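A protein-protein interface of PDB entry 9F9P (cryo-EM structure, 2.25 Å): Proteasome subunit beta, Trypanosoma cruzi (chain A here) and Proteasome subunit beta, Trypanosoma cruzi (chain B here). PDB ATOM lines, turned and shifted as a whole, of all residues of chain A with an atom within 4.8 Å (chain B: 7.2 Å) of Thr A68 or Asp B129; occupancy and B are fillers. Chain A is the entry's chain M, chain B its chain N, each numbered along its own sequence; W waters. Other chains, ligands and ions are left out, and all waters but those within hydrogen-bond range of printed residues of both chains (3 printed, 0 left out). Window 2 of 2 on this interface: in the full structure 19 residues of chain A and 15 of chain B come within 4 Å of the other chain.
Among the printed residues, merely in contact across the chains: Leu A60 with Trp B127 (3.9 Å) and His A67 with Trp B127 (3.8 Å).
Water W1 lies within hydrogen-bond range of the side-chain carboxylate (OD2) of Asp B129 (2.6 Å), the backbone NH (N) of Arg A69 (2.7 Å) and the side-chain hydroxyl (OG1) of Thr A68 (3.1 Å).
Water W2 lies within hydrogen-bond range of the backbone carbonyl oxygen (O) of His A67, the backbone carbonyl oxygen (O) of Cys B131 and the indole nitrogen (NE1) of Trp B127.
Water W3 lies within hydrogen-bond range of the backbone NH of Ile A66 (3.1 Å) and the guanidinium group of Arg B146 (3.2 Å).
Hydrophobic or aromatic side chains of chain B that line the printed part of chain A: Trp B127.
Among the printed residues, 5 pairs touch across the chains.
Among the printed residues, no Asp or Glu carboxylate lies within 4 Å of a Lys or Arg side-chain nitrogen of the other chain.
The backbone NH (N) of His A67 lies within hydrogen-bond range of the backbone carbonyl oxygen (O) of Leu A60 (2.9 Å).
O of Thr A68 sits at hydrogen-bond distance from N of Leu A60 (3.0 Å).
OG1 of Thr A68 is in hydrogen-bond range of N of Asp A70.
The backbone NH (N) of Gly B119 is in hydrogen-bond range of the backbone carbonyl oxygen (O) of Trp B127 (3.0 Å).
Of chain B, only Asp B129 (3.0 Å) comes within 4 Å of Thr A68.
Asp B129 touches just one residue of chain A: Thr A68 (3.0 Å).
Of the printed residues of chain A, Arg B146 touches Ile A66 (2.8 Å) and His A67 (3.4 Å).
Printed residues of chain A within 4 Å of Trp B127: Leu A60 and His A67.
Printed residues of chain B within 4 Å of His A67: Trp B127 (3.8 Å) and Arg B146 (3.4 Å).
Printed residues of chain B within 4 Å of Leu A60: Trp B127.
Of the printed residues of chain B, Ile A66 touches Arg B146 (2.8 Å).
Thr B128 touches none of the printed residues of chain A.
The nearest residue of chain A that does not touch Asp B129 is His A67 (4.04 Å).
The guanidinium group (NH2) of Arg B146 sits at hydrogen-bond distance from the backbone carbonyl oxygen (O) of Ile A66 (2.8 Å).
NH2 of Arg B146 is in hydrogen-bond range of O of His A67 (3.4 Å).
The side-chain hydroxyl (OG1) of Thr A68 lies within hydrogen-bond range of the side-chain carboxylate (OD2) of Asp B129, at 3.0 Å.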
ATOM      1  N   THR A  58     -18.595   6.296   3.658  1.00  0.00           N
ATOM      2  CA  THR A  58     -18.963   4.991   3.118  1.00  0.00           C
ATOM      3  C   THR A  58     -17.783   4.040   2.840  1.00  0.00           C
ATOM      4  O   THR A  58     -17.958   3.010   2.221  1.00  0.00           O
ATOM      5  CB  THR A  58     -19.706   5.163   1.782  1.00  0.00           C
ATOM      6  OG1 THR A  58     -18.880   5.677   0.732  1.00  0.00           O
ATOM      7  CG2 THR A  58     -20.919   6.063   1.918  1.00  0.00           C
ATOM      8  N   ARG A  59     -16.566   4.362   3.254  1.00  0.00           N
ATOM      9  CA  ARG A  59     -15.439   3.507   2.954  1.00  0.00           C
ATOM     10  C   ARG A  59     -15.286   2.439   4.035  1.00  0.00           C
ATOM     11  O   ARG A  59     -15.303   2.770   5.212  1.00  0.00           O
ATOM     12  CB  ARG A  59     -14.184   4.373   2.830  1.00  0.00           C
ATOM     13  CG  ARG A  59     -12.915   3.602   2.529  1.00  0.00           C
ATOM     14  CD  ARG A  59     -11.668   4.464   2.450  1.00  0.00           C
ATOM     15  NE  ARG A  59     -11.717   5.149   1.176  1.00  0.00           N
ATOM     16  CZ  ARG A  59     -10.807   6.008   0.769  1.00  0.00           C
ATOM     17  NH1 ARG A  59     -10.976   6.641  -0.380  1.00  0.00           N
ATOM     18  NH2 ARG A  59      -9.762   6.241   1.542  1.00  0.00           N
ATOM     19  N   LEU A  60     -15.054   1.194   3.651  1.00  0.00           N
ATOM     20  CA  LEU A  60     -14.693   0.154   4.607  1.00  0.00           C
ATOM     21  C   LEU A  60     -13.265  -0.341   4.353  1.00  0.00           C
ATOM     22  O   LEU A  60     -12.998  -0.961   3.339  1.00  0.00           O
ATOM     23  CB  LEU A  60     -15.724  -0.976   4.450  1.00  0.00           C
ATOM     24  CG  LEU A  60     -15.682  -2.146   5.428  1.00  0.00           C
ATOM     25  CD1 LEU A  60     -16.288  -1.713   6.730  1.00  0.00           C
ATOM     26  CD2 LEU A  60     -16.427  -3.386   4.908  1.00  0.00           C
ATOM     27  N   ILE A  66      -8.495  -1.658   0.937  1.00  0.00           N
ATOM     28  CA  ILE A  66      -9.877  -1.231   1.005  1.00  0.00           C
ATOM     29  C   ILE A  66     -10.800  -2.358   0.563  1.00  0.00           C
ATOM     30  O   ILE A  66     -10.704  -2.810  -0.561  1.00  0.00           O
ATOM     31  CB  ILE A  66     -10.019  -0.053   0.033  1.00  0.00           C
ATOM     32  CG1 ILE A  66      -9.330   1.203   0.555  1.00  0.00           C
ATOM     33  CG2 ILE A  66     -11.464   0.239  -0.324  1.00  0.00           C
ATOM     34  CD1 ILE A  66      -9.175   2.222  -0.555  1.00  0.00           C
ATOM     35  N   HIS A  67     -11.778  -2.726   1.379  1.00  0.00           N
ATOM     36  CA  HIS A  67     -12.725  -3.768   0.988  1.00  0.00           C
ATOM     37  C   HIS A  67     -13.755  -3.238   0.009  1.00  0.00           C
ATOM     38  O   HIS A  67     -14.007  -3.876  -1.001  1.00  0.00           O
ATOM     39  CB  HIS A  67     -13.423  -4.336   2.217  1.00  0.00           C
ATOM     40  CG  HIS A  67     -12.548  -5.095   3.142  1.00  0.00           C
ATOM     41  ND1 HIS A  67     -11.551  -5.953   2.733  1.00  0.00           N
ATOM     42  CD2 HIS A  67     -12.585  -5.133   4.499  1.00  0.00           C
ATOM     43  CE1 HIS A  67     -10.994  -6.485   3.846  1.00  0.00           C
ATOM     44  NE2 HIS A  67     -11.614  -6.000   4.942  1.00  0.00           N
ATOM     45  N   THR A  68     -14.327  -2.064   0.279  1.00  0.00           N
ATOM     46  CA  THR A  68     -15.331  -1.501  -0.608  1.00  0.00           C
ATOM     47  C   THR A  68     -15.436  -0.020  -0.355  1.00  0.00           C
ATOM     48  O   THR A  68     -15.199   0.413   0.743  1.00  0.00           O
ATOM     49  CB  THR A  68     -16.752  -2.108  -0.425  1.00  0.00           C
ATOM     50  OG1 THR A  68     -17.721  -1.497  -1.271  1.00  0.00           O
ATOM     51  CG2 THR A  68     -17.372  -1.907   0.954  1.00  0.00           C
ATOM     52  N   ARG A  69     -15.899   0.716  -1.345  1.00  0.00           N
ATOM     53  CA  ARG A  69     -16.141   2.138  -1.207  1.00  0.00           C
ATOM     54  C   ARG A  69     -17.616   2.477  -1.063  1.00  0.00           C
ATOM     55  O   ARG A  69     -17.967   3.636  -1.147  1.00  0.00           O
ATOM     56  CB  ARG A  69     -15.666   2.882  -2.450  1.00  0.00           C
ATOM     57  CG  ARG A  69     -14.178   2.775  -2.751  1.00  0.00           C
ATOM     58  CD  ARG A  69     -13.925   3.433  -4.118  1.00  0.00           C
ATOM     59  NE  ARG A  69     -12.597   3.155  -4.667  1.00  0.00           N
ATOM     60  CZ  ARG A  69     -11.464   3.670  -4.198  1.00  0.00           C
ATOM     61  NH1 ARG A  69     -10.301   3.255  -4.661  1.00  0.00           N
ATOM     62  NH2 ARG A  69     -11.499   4.582  -3.248  1.00  0.00           N
ATOM     63  N   ASP A  70     -18.483   1.507  -0.785  1.00  0.00           N
ATOM     64  CA  ASP A  70     -19.902   1.821  -0.713  1.00  0.00           C
ATOM     65  C   ASP A  70     -20.610   1.100   0.438  1.00  0.00           C
ATOM     66  O   ASP A  70     -21.744   0.682   0.277  1.00  0.00           O
ATOM     67  CB  ASP A  70     -20.522   1.502  -2.070  1.00  0.00           C
ATOM     68  CG  ASP A  70     -21.988   1.880  -2.205  1.00  0.00           C
ATOM     69  OD1 ASP A  70     -22.502   2.606  -1.309  1.00  0.00           O
ATOM     70  OD2 ASP A  70     -22.624   1.431  -3.212  1.00  0.00           O
ATOM     71  N   ASP A  71     -19.980   0.982   1.598  1.00  0.00           N
ATOM     72  CA  ASP A  71     -20.599   0.401   2.779  1.00  0.00           C
ATOM     73  C   ASP A  71     -21.636   1.353   3.401  1.00  0.00           C
ATOM     74  O   ASP A  71     -21.349   2.512   3.696  1.00  0.00           O
ATOM     75  CB  ASP A  71     -19.515   0.115   3.833  1.00  0.00           C
ATOM     76  CG  ASP A  71     -19.999  -0.404   5.194  1.00  0.00           C
ATOM     77  OD1 ASP A  71     -20.438  -1.583   5.246  1.00  0.00           O
ATOM     78  OD2 ASP A  71     -19.886   0.353   6.220  1.00  0.00           O
ATOM     79  N   GLY B   9     -13.220 -12.917  -7.536  1.00  0.00           N
ATOM     80  CA  GLY B   9     -14.531 -12.927  -8.178  1.00  0.00           C
ATOM     81  C   GLY B   9     -14.887 -11.593  -8.806  1.00  0.00           C
ATOM     82  O   GLY B   9     -14.466 -10.579  -8.256  1.00  0.00           O
ATOM     83  N   VAL B  10     -15.719 -11.595  -9.862  1.00  0.00           N
ATOM     84  CA  VAL B  10     -16.204 -10.347 -10.479  1.00  0.00           C
ATOM     85  C   VAL B  10     -17.585 -10.530 -11.076  1.00  0.00           C
ATOM     86  O   VAL B  10     -17.836 -11.537 -11.700  1.00  0.00           O
ATOM     87  CB  VAL B  10     -15.216  -9.875 -11.574  1.00  0.00           C
ATOM     88  CG1 VAL B  10     -15.041 -10.864 -12.734  1.00  0.00           C
ATOM     89  CG2 VAL B  10     -15.556  -8.519 -12.170  1.00  0.00           C
ATOM     90  N   LYS B  11     -18.448  -9.518 -10.958  1.00  0.00           N
ATOM     91  CA  LYS B  11     -19.752  -9.494 -11.630  1.00  0.00           C
ATOM     92  C   LYS B  11     -19.638  -8.946 -13.035  1.00  0.00           C
ATOM     93  O   LYS B  11     -18.922  -7.987 -13.257  1.00  0.00           O
ATOM     94  CB  LYS B  11     -20.731  -8.509 -10.984  1.00  0.00           C
ATOM     95  CG  LYS B  11     -21.110  -8.846  -9.573  1.00  0.00           C
ATOM     96  CD  LYS B  11     -22.317  -8.168  -9.055  1.00  0.00           C
ATOM     97  CE  LYS B  11     -22.393  -8.370  -7.547  1.00  0.00           C
ATOM     98  NZ  LYS B  11     -23.500  -7.614  -6.921  1.00  0.00           N
ATOM     99  N   VAL B  16     -21.923 -13.918 -12.564  1.00  0.00           N
ATOM    100  CA  VAL B  16     -20.759 -13.681 -11.751  1.00  0.00           C
ATOM    101  C   VAL B  16     -19.795 -14.846 -11.919  1.00  0.00           C
ATOM    102  O   VAL B  16     -20.206 -15.970 -12.132  1.00  0.00           O
ATOM    103  CB  VAL B  16     -21.126 -13.363 -10.273  1.00  0.00           C
ATOM    104  CG1 VAL B  16     -22.122 -14.320  -9.662  1.00  0.00           C
ATOM    105  CG2 VAL B  16     -19.903 -13.340  -9.348  1.00  0.00           C
ATOM    106  N   PHE B 116     -25.094 -12.229  -7.093  1.00  0.00           N
ATOM    107  CA  PHE B 116     -24.626 -11.891  -5.763  1.00  0.00           C
ATOM    108  C   PHE B 116     -23.113 -12.080  -5.641  1.00  0.00           C
ATOM    109  O   PHE B 116     -22.573 -13.026  -6.143  1.00  0.00           O
ATOM    110  CB  PHE B 116     -25.438 -12.749  -4.776  1.00  0.00           C
ATOM    111  CG  PHE B 116     -25.021 -12.555  -3.358  1.00  0.00           C
ATOM    112  CD1 PHE B 116     -25.562 -11.533  -2.622  1.00  0.00           C
ATOM    113  CD2 PHE B 116     -23.957 -13.284  -2.845  1.00  0.00           C
ATOM    114  CE1 PHE B 116     -25.131 -11.287  -1.342  1.00  0.00           C
ATOM    115  CE2 PHE B 116     -23.463 -12.991  -1.579  1.00  0.00           C
ATOM    116  CZ  PHE B 116     -24.090 -12.025  -0.807  1.00  0.00           C
ATOM    117  N   LEU B 117     -22.404 -11.234  -4.914  1.00  0.00           N
ATOM    118  CA  LEU B 117     -20.997 -11.476  -4.601  1.00  0.00           C
ATOM    119  C   LEU B 117     -20.656 -10.821  -3.286  1.00  0.00           C
ATOM    120  O   LEU B 117     -20.970  -9.670  -3.125  1.00  0.00           O
ATOM    121  CB  LEU B 117     -20.126 -10.884  -5.712  1.00  0.00           C
ATOM    122  CG  LEU B 117     -18.621 -11.146  -5.645  1.00  0.00           C
ATOM    123  CD1 LEU B 117     -18.282 -12.638  -5.717  1.00  0.00           C
ATOM    124  CD2 LEU B 117     -17.872 -10.376  -6.756  1.00  0.00           C
ATOM    125  N   GLY B 118     -19.986 -11.510  -2.373  1.00  0.00           N
ATOM    126  CA  GLY B 118     -19.673 -10.948  -1.067  1.00  0.00           C
ATOM    127  C   GLY B 118     -18.508 -11.623  -0.372  1.00  0.00           C
ATOM    128  O   GLY B 118     -18.191 -12.748  -0.694  1.00  0.00           O
ATOM    129  N   GLY B 119     -17.888 -10.958   0.593  1.00  0.00           N
ATOM    130  CA  GLY B 119     -16.848 -11.571   1.398  1.00  0.00           C
ATOM    131  C   GLY B 119     -17.120 -11.497   2.885  1.00  0.00           C
ATOM    132  O   GLY B 119     -17.806 -10.606   3.327  1.00  0.00           O
ATOM    133  N   ARG B 126     -18.259  -8.090   6.985  1.00  0.00           N
ATOM    134  CA  ARG B 126     -18.902  -8.513   5.763  1.00  0.00           C
ATOM    135  C   ARG B 126     -19.139  -7.365   4.799  1.00  0.00           C
ATOM    136  O   ARG B 126     -19.426  -6.286   5.227  1.00  0.00           O
ATOM    137  CB  ARG B 126     -20.229  -9.231   6.024  1.00  0.00           C
ATOM    138  CG  ARG B 126     -21.224  -8.482   6.893  1.00  0.00           C
ATOM    139  CD  ARG B 126     -22.624  -9.055   6.763  1.00  0.00           C
ATOM    140  NE  ARG B 126     -23.326  -8.522   5.620  1.00  0.00           N
ATOM    141  CZ  ARG B 126     -24.405  -9.088   5.087  1.00  0.00           C
ATOM    142  NH1 ARG B 126     -25.004 -10.099   5.694  1.00  0.00           N
ATOM    143  NH2 ARG B 126     -24.916  -8.616   3.959  1.00  0.00           N
ATOM    144  N   TRP B 127     -19.082  -7.660   3.505  1.00  0.00           N
ATOM    145  CA  TRP B 127     -19.258  -6.652   2.479  1.00  0.00           C
ATOM    146  C   TRP B 127     -19.703  -7.286   1.175  1.00  0.00           C
ATOM    147  O   TRP B 127     -19.395  -8.424   0.921  1.00  0.00           O
ATOM    148  CB  TRP B 127     -17.991  -5.806   2.258  1.00  0.00           C
ATOM    149  CG  TRP B 127     -16.813  -6.546   1.724  1.00  0.00           C
ATOM    150  CD1 TRP B 127     -16.380  -6.513   0.444  1.00  0.00           C
ATOM    151  CD2 TRP B 127     -15.863  -7.316   2.455  1.00  0.00           C
ATOM    152  NE1 TRP B 127     -15.320  -7.335   0.298  1.00  0.00           N
ATOM    153  CE2 TRP B 127     -14.964  -7.823   1.518  1.00  0.00           C
ATOM    154  CE3 TRP B 127     -15.733  -7.698   3.793  1.00  0.00           C
ATOM    155  CZ2 TRP B 127     -13.949  -8.700   1.845  1.00  0.00           C
ATOM    156  CZ3 TRP B 127     -14.718  -8.566   4.142  1.00  0.00           C
ATOM    157  CH2 TRP B 127     -13.843  -9.088   3.165  1.00  0.00           C
ATOM    158  N   THR B 128     -20.363  -6.494   0.337  1.00  0.00           N
ATOM    159  CA  THR B 128     -20.713  -6.910  -1.013  1.00  0.00           C
ATOM    160  C   THR B 128     -20.217  -5.905  -2.029  1.00  0.00           C
ATOM    161  O   THR B 128     -20.318  -4.729  -1.771  1.00  0.00           O
ATOM    162  CB  THR B 128     -22.244  -6.976  -1.217  1.00  0.00           C
ATOM    163  OG1 THR B 128     -22.867  -5.725  -0.870  1.00  0.00           O
ATOM    164  CG2 THR B 128     -22.930  -8.070  -0.421  1.00  0.00           C
ATOM    165  N   ASP B 129     -19.853  -6.317  -3.239  1.00  0.00           N
ATOM    166  CA  ASP B 129     -19.328  -5.372  -4.221  1.00  0.00           C
ATOM    167  C   ASP B 129     -19.267  -6.040  -5.580  1.00  0.00           C
ATOM    168  O   ASP B 129     -19.541  -7.216  -5.678  1.00  0.00           O
ATOM    169  CB  ASP B 129     -17.943  -4.858  -3.827  1.00  0.00           C
ATOM    170  CG  ASP B 129     -17.542  -3.511  -4.432  1.00  0.00           C
ATOM    171  OD1 ASP B 129     -18.129  -3.113  -5.499  1.00  0.00           O
ATOM    172  OD2 ASP B 129     -16.707  -2.800  -3.805  1.00  0.00           O
ATOM    173  N   ASP B 130     -18.945  -5.282  -6.624  1.00  0.00           N
ATOM    174  CA  ASP B 130     -18.757  -5.814  -7.958  1.00  0.00           C
ATOM    175  C   ASP B 130     -17.463  -6.618  -8.112  1.00  0.00           C
ATOM    176  O   ASP B 130     -17.401  -7.389  -9.044  1.00  0.00           O
ATOM    177  CB  ASP B 130     -18.746  -4.711  -9.002  1.00  0.00           C
ATOM    178  CG  ASP B 130     -20.083  -3.984  -9.224  1.00  0.00           C
ATOM    179  OD1 ASP B 130     -21.190  -4.562  -8.890  1.00  0.00           O
ATOM    180  OD2 ASP B 130     -20.026  -2.797  -9.744  1.00  0.00           O
ATOM    181  N   CYS B 131     -16.446  -6.430  -7.243  1.00  0.00           N
ATOM    182  CA  CYS B 131     -15.347  -7.368  -7.176  1.00  0.00           C
ATOM    183  C   CYS B 131     -14.861  -7.638  -5.769  1.00  0.00           C
ATOM    184  O   CYS B 131     -14.791  -6.741  -4.986  1.00  0.00           O
ATOM    185  CB  CYS B 131     -14.133  -6.933  -7.987  1.00  0.00           C
ATOM    186  SG  CYS B 131     -13.595  -5.226  -7.723  1.00  0.00           S
ATOM    187  N   VAL B 132     -14.486  -8.879  -5.502  1.00  0.00           N
ATOM    188  CA  VAL B 132     -14.163  -9.344  -4.177  1.00  0.00           C
ATOM    189  C   VAL B 132     -12.978 -10.304  -4.262  1.00  0.00           C
ATOM    190  O   VAL B 132     -12.900 -11.074  -5.195  1.00  0.00           O
ATOM    191  CB  VAL B 132     -15.408 -10.005  -3.513  1.00  0.00           C
ATOM    192  CG1 VAL B 132     -15.098 -10.648  -2.174  1.00  0.00           C
ATOM    193  CG2 VAL B 132     -16.555  -9.042  -3.279  1.00  0.00           C
ATOM    194  N   LEU B 142      -7.526  -7.084  -7.150  1.00  0.00           N
ATOM    195  CA  LEU B 142      -8.501  -6.022  -7.074  1.00  0.00           C
ATOM    196  C   LEU B 142      -8.106  -4.785  -7.872  1.00  0.00           C
ATOM    197  O   LEU B 142      -8.976  -4.204  -8.518  1.00  0.00           O
ATOM    198  CB  LEU B 142      -8.769  -5.626  -5.613  1.00  0.00           C
ATOM    199  CG  LEU B 142      -9.577  -6.633  -4.810  1.00  0.00           C
ATOM    200  CD1 LEU B 142      -9.815  -6.133  -3.419  1.00  0.00           C
ATOM    201  CD2 LEU B 142     -10.907  -6.939  -5.477  1.00  0.00           C
ATOM    202  N   ARG B 146     -10.863  -3.541 -10.545  1.00  0.00           N
ATOM    203  CA  ARG B 146     -11.464  -2.235 -10.339  1.00  0.00           C
ATOM    204  C   ARG B 146     -11.276  -1.286 -11.519  1.00  0.00           C
ATOM    205  O   ARG B 146     -12.209  -0.557 -11.850  1.00  0.00           O
ATOM    206  CB  ARG B 146     -10.932  -1.545  -9.089  1.00  0.00           C
ATOM    207  CG  ARG B 146     -11.612  -2.003  -7.818  1.00  0.00           C
ATOM    208  CD  ARG B 146     -10.770  -1.762  -6.601  1.00  0.00           C
ATOM    209  NE  ARG B 146     -11.463  -2.202  -5.397  1.00  0.00           N
ATOM    210  CZ  ARG B 146     -10.886  -2.333  -4.211  1.00  0.00           C
ATOM    211  NH1 ARG B 146      -9.632  -1.954  -4.005  1.00  0.00           N
ATOM    212  NH2 ARG B 146     -11.561  -2.893  -3.225  1.00  0.00           N
ATOM    213  N   LEU B 149     -13.800  -2.403 -14.296  1.00  0.00           N
ATOM    214  CA  LEU B 149     -15.185  -2.018 -13.997  1.00  0.00           C
ATOM    215  C   LEU B 149     -15.431  -0.510 -14.120  1.00  0.00           C
ATOM    216  O   LEU B 149     -16.541  -0.073 -13.866  1.00  0.00           O
ATOM    217  CB  LEU B 149     -15.532  -2.488 -12.584  1.00  0.00           C
ATOM    218  CG  LEU B 149     -15.659  -3.994 -12.401  1.00  0.00           C
ATOM    219  CD1 LEU B 149     -15.524  -4.372 -10.933  1.00  0.00           C
ATOM    220  CD2 LEU B 149     -16.977  -4.497 -12.912  1.00  0.00           C
HETATM  221  O   HOH W   1     -16.565  -0.223  -3.790  1.00  0.00           O
HETATM  222  O   HOH W   2     -14.006  -6.110  -2.477  1.00  0.00           O
HETATM  223  O   HOH W   3      -7.249  -1.774  -1.875  1.00  0.00           O
